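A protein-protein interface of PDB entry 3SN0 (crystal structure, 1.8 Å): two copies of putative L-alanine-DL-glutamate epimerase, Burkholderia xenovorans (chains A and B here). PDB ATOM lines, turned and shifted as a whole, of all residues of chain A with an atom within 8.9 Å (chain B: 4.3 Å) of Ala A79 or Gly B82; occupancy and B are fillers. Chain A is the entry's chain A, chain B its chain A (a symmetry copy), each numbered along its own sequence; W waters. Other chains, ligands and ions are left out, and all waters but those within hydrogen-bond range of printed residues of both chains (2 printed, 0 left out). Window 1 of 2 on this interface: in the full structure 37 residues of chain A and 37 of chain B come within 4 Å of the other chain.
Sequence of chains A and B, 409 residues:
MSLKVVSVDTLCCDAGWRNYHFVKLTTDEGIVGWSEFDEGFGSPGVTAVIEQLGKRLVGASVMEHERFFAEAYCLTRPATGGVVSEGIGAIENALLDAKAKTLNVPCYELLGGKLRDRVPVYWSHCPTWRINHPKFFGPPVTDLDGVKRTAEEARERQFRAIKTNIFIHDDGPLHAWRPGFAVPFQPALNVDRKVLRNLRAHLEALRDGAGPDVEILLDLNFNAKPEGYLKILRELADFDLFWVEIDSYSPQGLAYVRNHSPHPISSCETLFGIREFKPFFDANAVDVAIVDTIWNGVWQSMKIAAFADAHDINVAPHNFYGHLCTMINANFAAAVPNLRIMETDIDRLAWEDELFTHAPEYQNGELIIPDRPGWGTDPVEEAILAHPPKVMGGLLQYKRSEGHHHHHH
Of the 19 printed residues of chain A, 6 touch a printed residue of chain B. Printed residues of chain A that touch a printed residue of chain B: Leu A75, Thr A76, Pro A78, Ala A79, Val A83 and Val A84. Hydrophobic or aromatic side chains of chain A that line the printed part of chain B: Pro A78, Ala A79, Val A83 and Val A84. Of the 10 printed residues of chain B, 7 touch a printed residue of chain A. Hydrophobic or aromatic side chains of chain B within 4 Å of the printed part of chain A: Val B83, Val B84 and Trp B295. Along chain B the printed residues that touch a printed residue of chain A span positions 42 to 295. Among the printed residues, 9 pairs touch across the chains. Among the printed residues, no Asp or Glu carboxylate lies within 4 Å of a Lys or Arg side-chain nitrogen of the other chain.
Printed residues of chain B within 4 Å of Ala A79: Gly B42, Ser B43, Gly B82 and Glu B86. Of the printed residues of chain A, Gly B82 touches Ala A79 (3.99 Å). No residue of chain A comes within 4 Å of Ser B85. Printed residues of chain A within 4 Å of Val B83: Val A84. Of the printed residues of chain A, Ser B43 touches Ala A79. Printed residues of chain A within 4 Å of Trp B295: Pro A78. Pro A44 touches none of the printed residues of chain B. The nearest printed residue of chain A that does not touch Gly B82 is Thr A80 (4.6 Å). The nearest printed residue of chain B that does not touch Leu A75 is Ser B43 (5.5 Å).
Water W1 lies within hydrogen-bond range of the backbone carbonyl oxygen of Ala A79 (2.8 Å), the backbone carbonyl oxygen of Gly A81 (2.9 Å), the backbone NH of Val B83 (2.9 Å) and the backbone NH of Val A84 (3.2 Å). Water W2 lies within hydrogen-bond range of the backbone carbonyl oxygen (O) of Gly B81 (2.9 Å), the backbone NH (N) of Val A83 (2.9 Å) and the backbone NH (N) of Val B84 (3.2 Å).
CA of Gly B42 touches O of Leu A75 (3.5 Å). CB of Thr A76 touches O of Gly B42, 3.6 Å away. Pro A78 touches Trp B295 (O to CZ3, 3.4 Å). O of Gly B42 touches CB of Ala A79, 3.4 Å away. Ala A79 touches Ser B43. Ala A79 touches Gly B82. Ala A79 touches Glu B86 (CB to OE2, 3.5 Å). CG2 of Val B84 touches CG2 of Val A83, 3.7 Å away. CG2 of Val B83 touches CG2 of Val A84, at 3.7 Å.
Val A83 touches Val B84, and with the chains exchanged Val A84 touches Val B83. Of the 9 pairs that touch across the chains among the printed residues, 2 have their exchanged pair printed and touching as well.
O of Ala A72 sits at hydrogen-bond distance from OG1 of Thr A76. The side-chain carboxylate (OE2) of Glu B86 lies within hydrogen-bond range of the side-chain hydroxyl (OG) of Ser B43, 2.6 Å away. The side-chain carboxylate (OE1) of Glu B86 is in hydrogen-bond range of the indole nitrogen (NE1) of Trp B295 (3.3 Å).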
ATOM      1  N   PRO A  44       0.473  21.033   4.354  1.00  0.00           N
ATOM      2  CA  PRO A  44      -0.464  22.131   4.391  1.00  0.00           C
ATOM      3  C   PRO A  44       0.331  23.415   4.556  1.00  0.00           C
ATOM      4  O   PRO A  44       1.352  23.409   5.272  1.00  0.00           O
ATOM      5  CB  PRO A  44      -1.283  21.846   5.661  1.00  0.00           C
ATOM      6  CG  PRO A  44      -0.416  21.018   6.481  1.00  0.00           C
ATOM      7  CD  PRO A  44       0.401  20.217   5.579  1.00  0.00           C
ATOM      8  N   VAL A  49       2.770  30.238   1.940  1.00  0.00           N
ATOM      9  CA  VAL A  49       4.163  30.625   1.837  1.00  0.00           C
ATOM     10  C   VAL A  49       4.401  31.337   0.508  1.00  0.00           C
ATOM     11  O   VAL A  49       5.018  32.416   0.451  1.00  0.00           O
ATOM     12  CB  VAL A  49       5.103  29.383   1.920  1.00  0.00           C
ATOM     13  CG1 VAL A  49       6.537  29.774   1.632  1.00  0.00           C
ATOM     14  CG2 VAL A  49       4.950  28.688   3.269  1.00  0.00           C
ATOM     15  N   ALA A  72      14.936  34.894  -0.198  1.00  0.00           N
ATOM     16  CA  ALA A  72      13.855  34.141   0.443  1.00  0.00           C
ATOM     17  C   ALA A  72      14.363  33.294   1.596  1.00  0.00           C
ATOM     18  O   ALA A  72      13.726  33.211   2.652  1.00  0.00           O
ATOM     19  CB  ALA A  72      13.120  33.263  -0.593  1.00  0.00           C
ATOM     20  N   TYR A  73      15.507  32.661   1.396  1.00  0.00           N
ATOM     21  CA  TYR A  73      16.146  31.904   2.454  1.00  0.00           C
ATOM     22  C   TYR A  73      16.415  32.777   3.680  1.00  0.00           C
ATOM     23  O   TYR A  73      16.099  32.376   4.796  1.00  0.00           O
ATOM     24  CB  TYR A  73      17.435  31.282   1.951  1.00  0.00           C
ATOM     25  CG  TYR A  73      18.093  30.403   2.995  1.00  0.00           C
ATOM     26  CD1 TYR A  73      17.551  29.167   3.340  1.00  0.00           C
ATOM     27  CD2 TYR A  73      19.247  30.799   3.622  1.00  0.00           C
ATOM     28  CE1 TYR A  73      18.162  28.354   4.310  1.00  0.00           C
ATOM     29  CE2 TYR A  73      19.866  29.998   4.593  1.00  0.00           C
ATOM     30  CZ  TYR A  73      19.322  28.784   4.927  1.00  0.00           C
ATOM     31  OH  TYR A  73      19.934  28.011   5.874  1.00  0.00           O
ATOM     32  N   CYS A  74      16.962  33.977   3.463  1.00  0.00           N
ATOM     33  CA  CYS A  74      17.165  34.949   4.536  1.00  0.00           C
ATOM     34  C   CYS A  74      15.876  35.280   5.267  1.00  0.00           C
ATOM     35  O   CYS A  74      15.836  35.252   6.499  1.00  0.00           O
ATOM     36  CB  CYS A  74      17.773  36.251   4.007  1.00  0.00           C
ATOM     37  SG  CYS A  74      19.517  36.117   3.476  1.00  0.00           S
ATOM     38  N   LEU A  75      14.826  35.596   4.504  1.00  0.00           N
ATOM     39  CA  LEU A  75      13.575  36.060   5.086  1.00  0.00           C
ATOM     40  C   LEU A  75      12.796  34.969   5.846  1.00  0.00           C
ATOM     41  O   LEU A  75      11.897  35.295   6.622  1.00  0.00           O
ATOM     42  CB  LEU A  75      12.682  36.660   4.016  1.00  0.00           C
ATOM     43  CG  LEU A  75      13.201  37.941   3.364  1.00  0.00           C
ATOM     44  CD1 LEU A  75      12.279  38.356   2.207  1.00  0.00           C
ATOM     45  CD2 LEU A  75      13.315  39.059   4.395  1.00  0.00           C
ATOM     46  N   THR A  76      13.098  33.701   5.584  1.00  0.00           N
ATOM     47  CA  THR A  76      12.440  32.570   6.251  1.00  0.00           C
ATOM     48  C   THR A  76      13.440  31.681   6.993  1.00  0.00           C
ATOM     49  O   THR A  76      13.109  30.554   7.380  1.00  0.00           O
ATOM     50  CB  THR A  76      11.644  31.699   5.240  1.00  0.00           C
ATOM     51  OG1 THR A  76      12.526  31.175   4.233  1.00  0.00           O
ATOM     52  CG2 THR A  76      10.507  32.529   4.557  1.00  0.00           C
ATOM     53  N   ARG A  77      14.644  32.195   7.223  1.00  0.00           N
ATOM     54  CA  ARG A  77      15.729  31.389   7.789  1.00  0.00           C
ATOM     55  C   ARG A  77      15.315  30.581   9.046  1.00  0.00           C
ATOM     56  O   ARG A  77      15.643  29.403   9.142  1.00  0.00           O
ATOM     57  CB  ARG A  77      16.942  32.289   8.074  1.00  0.00           C
ATOM     58  CG  ARG A  77      18.244  31.733   7.624  1.00  0.00           C
ATOM     59  CD  ARG A  77      19.390  32.683   7.961  1.00  0.00           C
ATOM     60  NE  ARG A  77      20.617  32.195   7.341  1.00  0.00           N
ATOM     61  CZ  ARG A  77      21.255  32.781   6.337  1.00  0.00           C
ATOM     62  NH1 ARG A  77      20.861  33.954   5.839  1.00  0.00           N
ATOM     63  NH2 ARG A  77      22.316  32.184   5.831  1.00  0.00           N
ATOM     64  N   PRO A  78      14.601  31.204   9.996  1.00  0.00           N
ATOM     65  CA  PRO A  78      14.279  30.475  11.233  1.00  0.00           C
ATOM     66  C   PRO A  78      13.418  29.216  11.069  1.00  0.00           C
ATOM     67  O   PRO A  78      13.557  28.270  11.870  1.00  0.00           O
ATOM     68  CB  PRO A  78      13.587  31.524  12.099  1.00  0.00           C
ATOM     69  CG  PRO A  78      14.106  32.848  11.582  1.00  0.00           C
ATOM     70  CD  PRO A  78      14.230  32.632  10.101  1.00  0.00           C
ATOM     71  N   ALA A  79      12.530  29.216  10.084  1.00  0.00           N
ATOM     72  CA  ALA A  79      11.585  28.110   9.866  1.00  0.00           C
ATOM     73  C   ALA A  79      11.831  27.443   8.504  1.00  0.00           C
ATOM     74  O   ALA A  79      10.909  26.932   7.865  1.00  0.00           O
ATOM     75  CB  ALA A  79      10.149  28.648   9.933  1.00  0.00           C
ATOM     76  N   THR A  80      13.085  27.419   8.081  1.00  0.00           N
ATOM     77  CA  THR A  80      13.460  26.823   6.805  1.00  0.00           C
ATOM     78  C   THR A  80      13.238  25.300   6.819  1.00  0.00           C
ATOM     79  O   THR A  80      13.131  24.648   7.897  1.00  0.00           O
ATOM     80  CB  THR A  80      14.911  27.144   6.425  1.00  0.00           C
ATOM     81  OG1 THR A  80      15.084  26.931   5.021  1.00  0.00           O
ATOM     82  CG2 THR A  80      15.919  26.266   7.231  1.00  0.00           C
ATOM     83  N   GLY A  81      13.149  24.745   5.622  1.00  0.00           N
ATOM     84  CA  GLY A  81      12.824  23.324   5.452  1.00  0.00           C
ATOM     85  C   GLY A  81      11.342  23.176   5.263  1.00  0.00           C
ATOM     86  O   GLY A  81      10.606  24.149   5.322  1.00  0.00           O
ATOM     87  N   GLY A  82      10.886  21.961   5.029  1.00  0.00           N
ATOM     88  CA  GLY A  82       9.463  21.699   4.982  1.00  0.00           C
ATOM     89  C   GLY A  82       8.657  22.602   4.068  1.00  0.00           C
ATOM     90  O   GLY A  82       9.045  22.862   2.912  1.00  0.00           O
ATOM     91  N   VAL A  83       7.517  23.055   4.577  1.00  0.00           N
ATOM     92  CA  VAL A  83       6.540  23.789   3.770  1.00  0.00           C
ATOM     93  C   VAL A  83       7.114  25.116   3.258  1.00  0.00           C
ATOM     94  O   VAL A  83       6.863  25.505   2.107  1.00  0.00           O
ATOM     95  CB  VAL A  83       5.218  23.928   4.550  1.00  0.00           C
ATOM     96  CG1 VAL A  83       4.361  25.063   4.025  1.00  0.00           C
ATOM     97  CG2 VAL A  83       4.455  22.576   4.482  1.00  0.00           C
ATOM     98  N   VAL A  84       7.893  25.793   4.098  1.00  0.00           N
ATOM     99  CA  VAL A  84       8.579  27.006   3.674  1.00  0.00           C
ATOM    100  C   VAL A  84       9.461  26.725   2.462  1.00  0.00           C
ATOM    101  O   VAL A  84       9.388  27.406   1.437  1.00  0.00           O
ATOM    102  CB  VAL A  84       9.401  27.637   4.824  1.00  0.00           C
ATOM    103  CG1 VAL A  84      10.450  28.641   4.275  1.00  0.00           C
ATOM    104  CG2 VAL A  84       8.470  28.324   5.823  1.00  0.00           C
ATOM    105  N   SER A  85      10.303  25.698   2.564  1.00  0.00           N
ATOM    106  CA  SER A  85      11.196  25.389   1.465  1.00  0.00           C
ATOM    107  C   SER A  85      10.457  24.900   0.221  1.00  0.00           C
ATOM    108  O   SER A  85      10.895  25.187  -0.898  1.00  0.00           O
ATOM    109  CB  SER A  85      12.265  24.385   1.897  1.00  0.00           C
ATOM    110  OG  SER A  85      13.202  25.038   2.736  1.00  0.00           O
ATOM    111  N   GLU A  86       9.327  24.208   0.396  1.00  0.00           N
ATOM    112  CA  GLU A  86       8.483  23.836  -0.755  1.00  0.00           C
ATOM    113  C   GLU A  86       7.937  25.058  -1.510  1.00  0.00           C
ATOM    114  O   GLU A  86       7.868  25.069  -2.758  1.00  0.00           O
ATOM    115  CB  GLU A  86       7.309  22.949  -0.314  1.00  0.00           C
ATOM    116  CG  GLU A  86       7.687  21.546   0.157  1.00  0.00           C
ATOM    117  CD  GLU A  86       6.468  20.735   0.557  1.00  0.00           C
ATOM    118  OE1 GLU A  86       5.516  20.685  -0.244  1.00  0.00           O
ATOM    119  OE2 GLU A  86       6.432  20.194   1.694  1.00  0.00           O
ATOM    120  N   ILE A  88       9.342  28.037  -1.619  1.00  0.00           N
ATOM    121  CA  ILE A  88      10.505  28.624  -2.294  1.00  0.00           C
ATOM    122  C   ILE A  88      10.845  27.837  -3.575  1.00  0.00           C
ATOM    123  O   ILE A  88      11.138  28.424  -4.626  1.00  0.00           O
ATOM    124  CB  ILE A  88      11.730  28.714  -1.348  1.00  0.00           C
ATOM    125  CG1 ILE A  88      11.466  29.738  -0.228  1.00  0.00           C
ATOM    126  CG2 ILE A  88      12.979  29.114  -2.119  1.00  0.00           C
ATOM    127  CD1 ILE A  88      12.507  29.703   0.887  1.00  0.00           C
ATOM    128  N   GLU A 276      20.586  18.775   4.454  1.00  0.00           N
ATOM    129  CA  GLU A 276      19.833  17.642   4.995  1.00  0.00           C
ATOM    130  C   GLU A 276      20.293  16.296   4.453  1.00  0.00           C
ATOM    131  O   GLU A 276      20.129  15.300   5.127  1.00  0.00           O
ATOM    132  CB  GLU A 276      18.320  17.812   4.794  1.00  0.00           C
ATOM    133  CG  GLU A 276      17.748  18.935   5.648  1.00  0.00           C
ATOM    134  CD  GLU A 276      16.219  19.024   5.638  1.00  0.00           C
ATOM    135  OE1 GLU A 276      15.544  18.202   4.968  1.00  0.00           O
ATOM    136  OE2 GLU A 276      15.699  19.941   6.310  1.00  0.00           O
ATOM    137  N   GLY B  42       9.748  34.473  10.179  1.00  0.00           N
ATOM    138  CA  GLY B  42      10.093  33.602   9.060  1.00  0.00           C
ATOM    139  C   GLY B  42       9.151  32.435   8.804  1.00  0.00           C
ATOM    140  O   GLY B  42       9.537  31.483   8.127  1.00  0.00           O
ATOM    141  N   SER B  43       7.899  32.559   9.264  1.00  0.00           N
ATOM    142  CA  SER B  43       6.995  31.418   9.384  1.00  0.00           C
ATOM    143  C   SER B  43       5.608  31.639   8.752  1.00  0.00           C
ATOM    144  O   SER B  43       4.583  31.474   9.433  1.00  0.00           O
ATOM    145  CB  SER B  43       6.829  31.094  10.876  1.00  0.00           C
ATOM    146  OG  SER B  43       8.089  30.740  11.484  1.00  0.00           O
ATOM    147  N   GLY B  81       8.854  19.577  10.774  1.00  0.00           N
ATOM    148  CA  GLY B  81       9.760  20.682  11.111  1.00  0.00           C
ATOM    149  C   GLY B  81       9.132  21.980  10.695  1.00  0.00           C
ATOM    150  O   GLY B  81       8.057  21.996  10.116  1.00  0.00           O
ATOM    151  N   GLY B  82       9.791  23.085  10.987  1.00  0.00           N
ATOM    152  CA  GLY B  82       9.339  24.370  10.497  1.00  0.00           C
ATOM    153  C   GLY B  82       7.882  24.701  10.761  1.00  0.00           C
ATOM    154  O   GLY B  82       7.370  24.508  11.881  1.00  0.00           O
ATOM    155  N   VAL B  83       7.222  25.229   9.737  1.00  0.00           N
ATOM    156  CA  VAL B  83       5.868  25.767   9.875  1.00  0.00           C
ATOM    157  C   VAL B  83       4.864  24.674  10.264  1.00  0.00           C
ATOM    158  O   VAL B  83       3.965  24.911  11.085  1.00  0.00           O
ATOM    159  CB  VAL B  83       5.487  26.555   8.606  1.00  0.00           C
ATOM    160  CG1 VAL B  83       3.986  26.707   8.456  1.00  0.00           C
ATOM    161  CG2 VAL B  83       6.185  27.943   8.656  1.00  0.00           C
ATOM    162  N   VAL B  84       5.028  23.482   9.694  1.00  0.00           N
ATOM    163  CA  VAL B  84       4.202  22.346  10.078  1.00  0.00           C
ATOM    164  C   VAL B  84       4.316  22.083  11.576  1.00  0.00           C
ATOM    165  O   VAL B  84       3.319  21.986  12.294  1.00  0.00           O
ATOM    166  CB  VAL B  84       4.550  21.077   9.263  1.00  0.00           C
ATOM    167  CG1 VAL B  84       4.000  19.801   9.956  1.00  0.00           C
ATOM    168  CG2 VAL B  84       4.004  21.195   7.841  1.00  0.00           C
ATOM    169  N   SER B  85       5.550  21.979  12.068  1.00  0.00           N
ATOM    170  CA  SER B  85       5.738  21.698  13.478  1.00  0.00           C
ATOM    171  C   SER B  85       5.275  22.843  14.377  1.00  0.00           C
ATOM    172  O   SER B  85       4.779  22.587  15.480  1.00  0.00           O
ATOM    173  CB  SER B  85       7.192  21.326  13.770  1.00  0.00           C
ATOM    174  OG  SER B  85       7.446  20.023  13.272  1.00  0.00           O
ATOM    175  N   GLU B  86       5.387  24.090  13.910  1.00  0.00           N
ATOM    176  CA  GLU B  86       4.823  25.230  14.657  1.00  0.00           C
ATOM    177  C   GLU B  86       3.298  25.137  14.819  1.00  0.00           C
ATOM    178  O   GLU B  86       2.739  25.468  15.887  1.00  0.00           O
ATOM    179  CB  GLU B  86       5.179  26.562  13.982  1.00  0.00           C
ATOM    180  CG  GLU B  86       6.655  26.954  14.042  1.00  0.00           C
ATOM    181  CD  GLU B  86       6.914  28.289  13.367  1.00  0.00           C
ATOM    182  OE1 GLU B  86       6.192  29.252  13.688  1.00  0.00           O
ATOM    183  OE2 GLU B  86       7.798  28.368  12.473  1.00  0.00           O
ATOM    184  N   PHE B 272      13.588  22.070  16.254  1.00  0.00           N
ATOM    185  CA  PHE B 272      12.419  21.297  16.644  1.00  0.00           C
ATOM    186  C   PHE B 272      12.763  19.871  17.049  1.00  0.00           C
ATOM    187  O   PHE B 272      13.324  19.133  16.261  1.00  0.00           O
ATOM    188  CB  PHE B 272      11.443  21.205  15.477  1.00  0.00           C
ATOM    189  CG  PHE B 272      10.896  22.501  15.025  1.00  0.00           C
ATOM    190  CD1 PHE B 272       9.654  22.919  15.437  1.00  0.00           C
ATOM    191  CD2 PHE B 272      11.606  23.285  14.120  1.00  0.00           C
ATOM    192  CE1 PHE B 272       9.136  24.127  14.993  1.00  0.00           C
ATOM    193  CE2 PHE B 272      11.099  24.494  13.676  1.00  0.00           C
ATOM    194  CZ  PHE B 272       9.871  24.909  14.106  1.00  0.00           C
ATOM    195  N   TRP B 295       6.886  27.352  19.520  1.00  0.00           N
ATOM    196  CA  TRP B 295       7.067  26.553  18.321  1.00  0.00           C
ATOM    197  C   TRP B 295       6.867  25.045  18.530  1.00  0.00           C
ATOM    198  O   TRP B 295       6.158  24.395  17.773  1.00  0.00           O
ATOM    199  CB  TRP B 295       8.483  26.801  17.778  1.00  0.00           C
ATOM    200  CG  TRP B 295       8.613  28.050  17.010  1.00  0.00           C
ATOM    201  CD1 TRP B 295       7.788  29.137  17.037  1.00  0.00           C
ATOM    202  CD2 TRP B 295       9.595  28.317  16.004  1.00  0.00           C
ATOM    203  NE1 TRP B 295       8.233  30.094  16.132  1.00  0.00           N
ATOM    204  CE2 TRP B 295       9.330  29.603  15.484  1.00  0.00           C
ATOM    205  CE3 TRP B 295      10.690  27.603  15.513  1.00  0.00           C
ATOM    206  CZ2 TRP B 295      10.105  30.178  14.469  1.00  0.00           C
ATOM    207  CZ3 TRP B 295      11.452  28.174  14.498  1.00  0.00           C
ATOM    208  CH2 TRP B 295      11.158  29.451  13.998  1.00  0.00           C
HETATM  209  O   HOH W   1       8.704  25.327   7.197  1.00  0.00           O
HETATM  210  O   HOH W   2       7.050  22.403   7.407  1.00  0.00           O
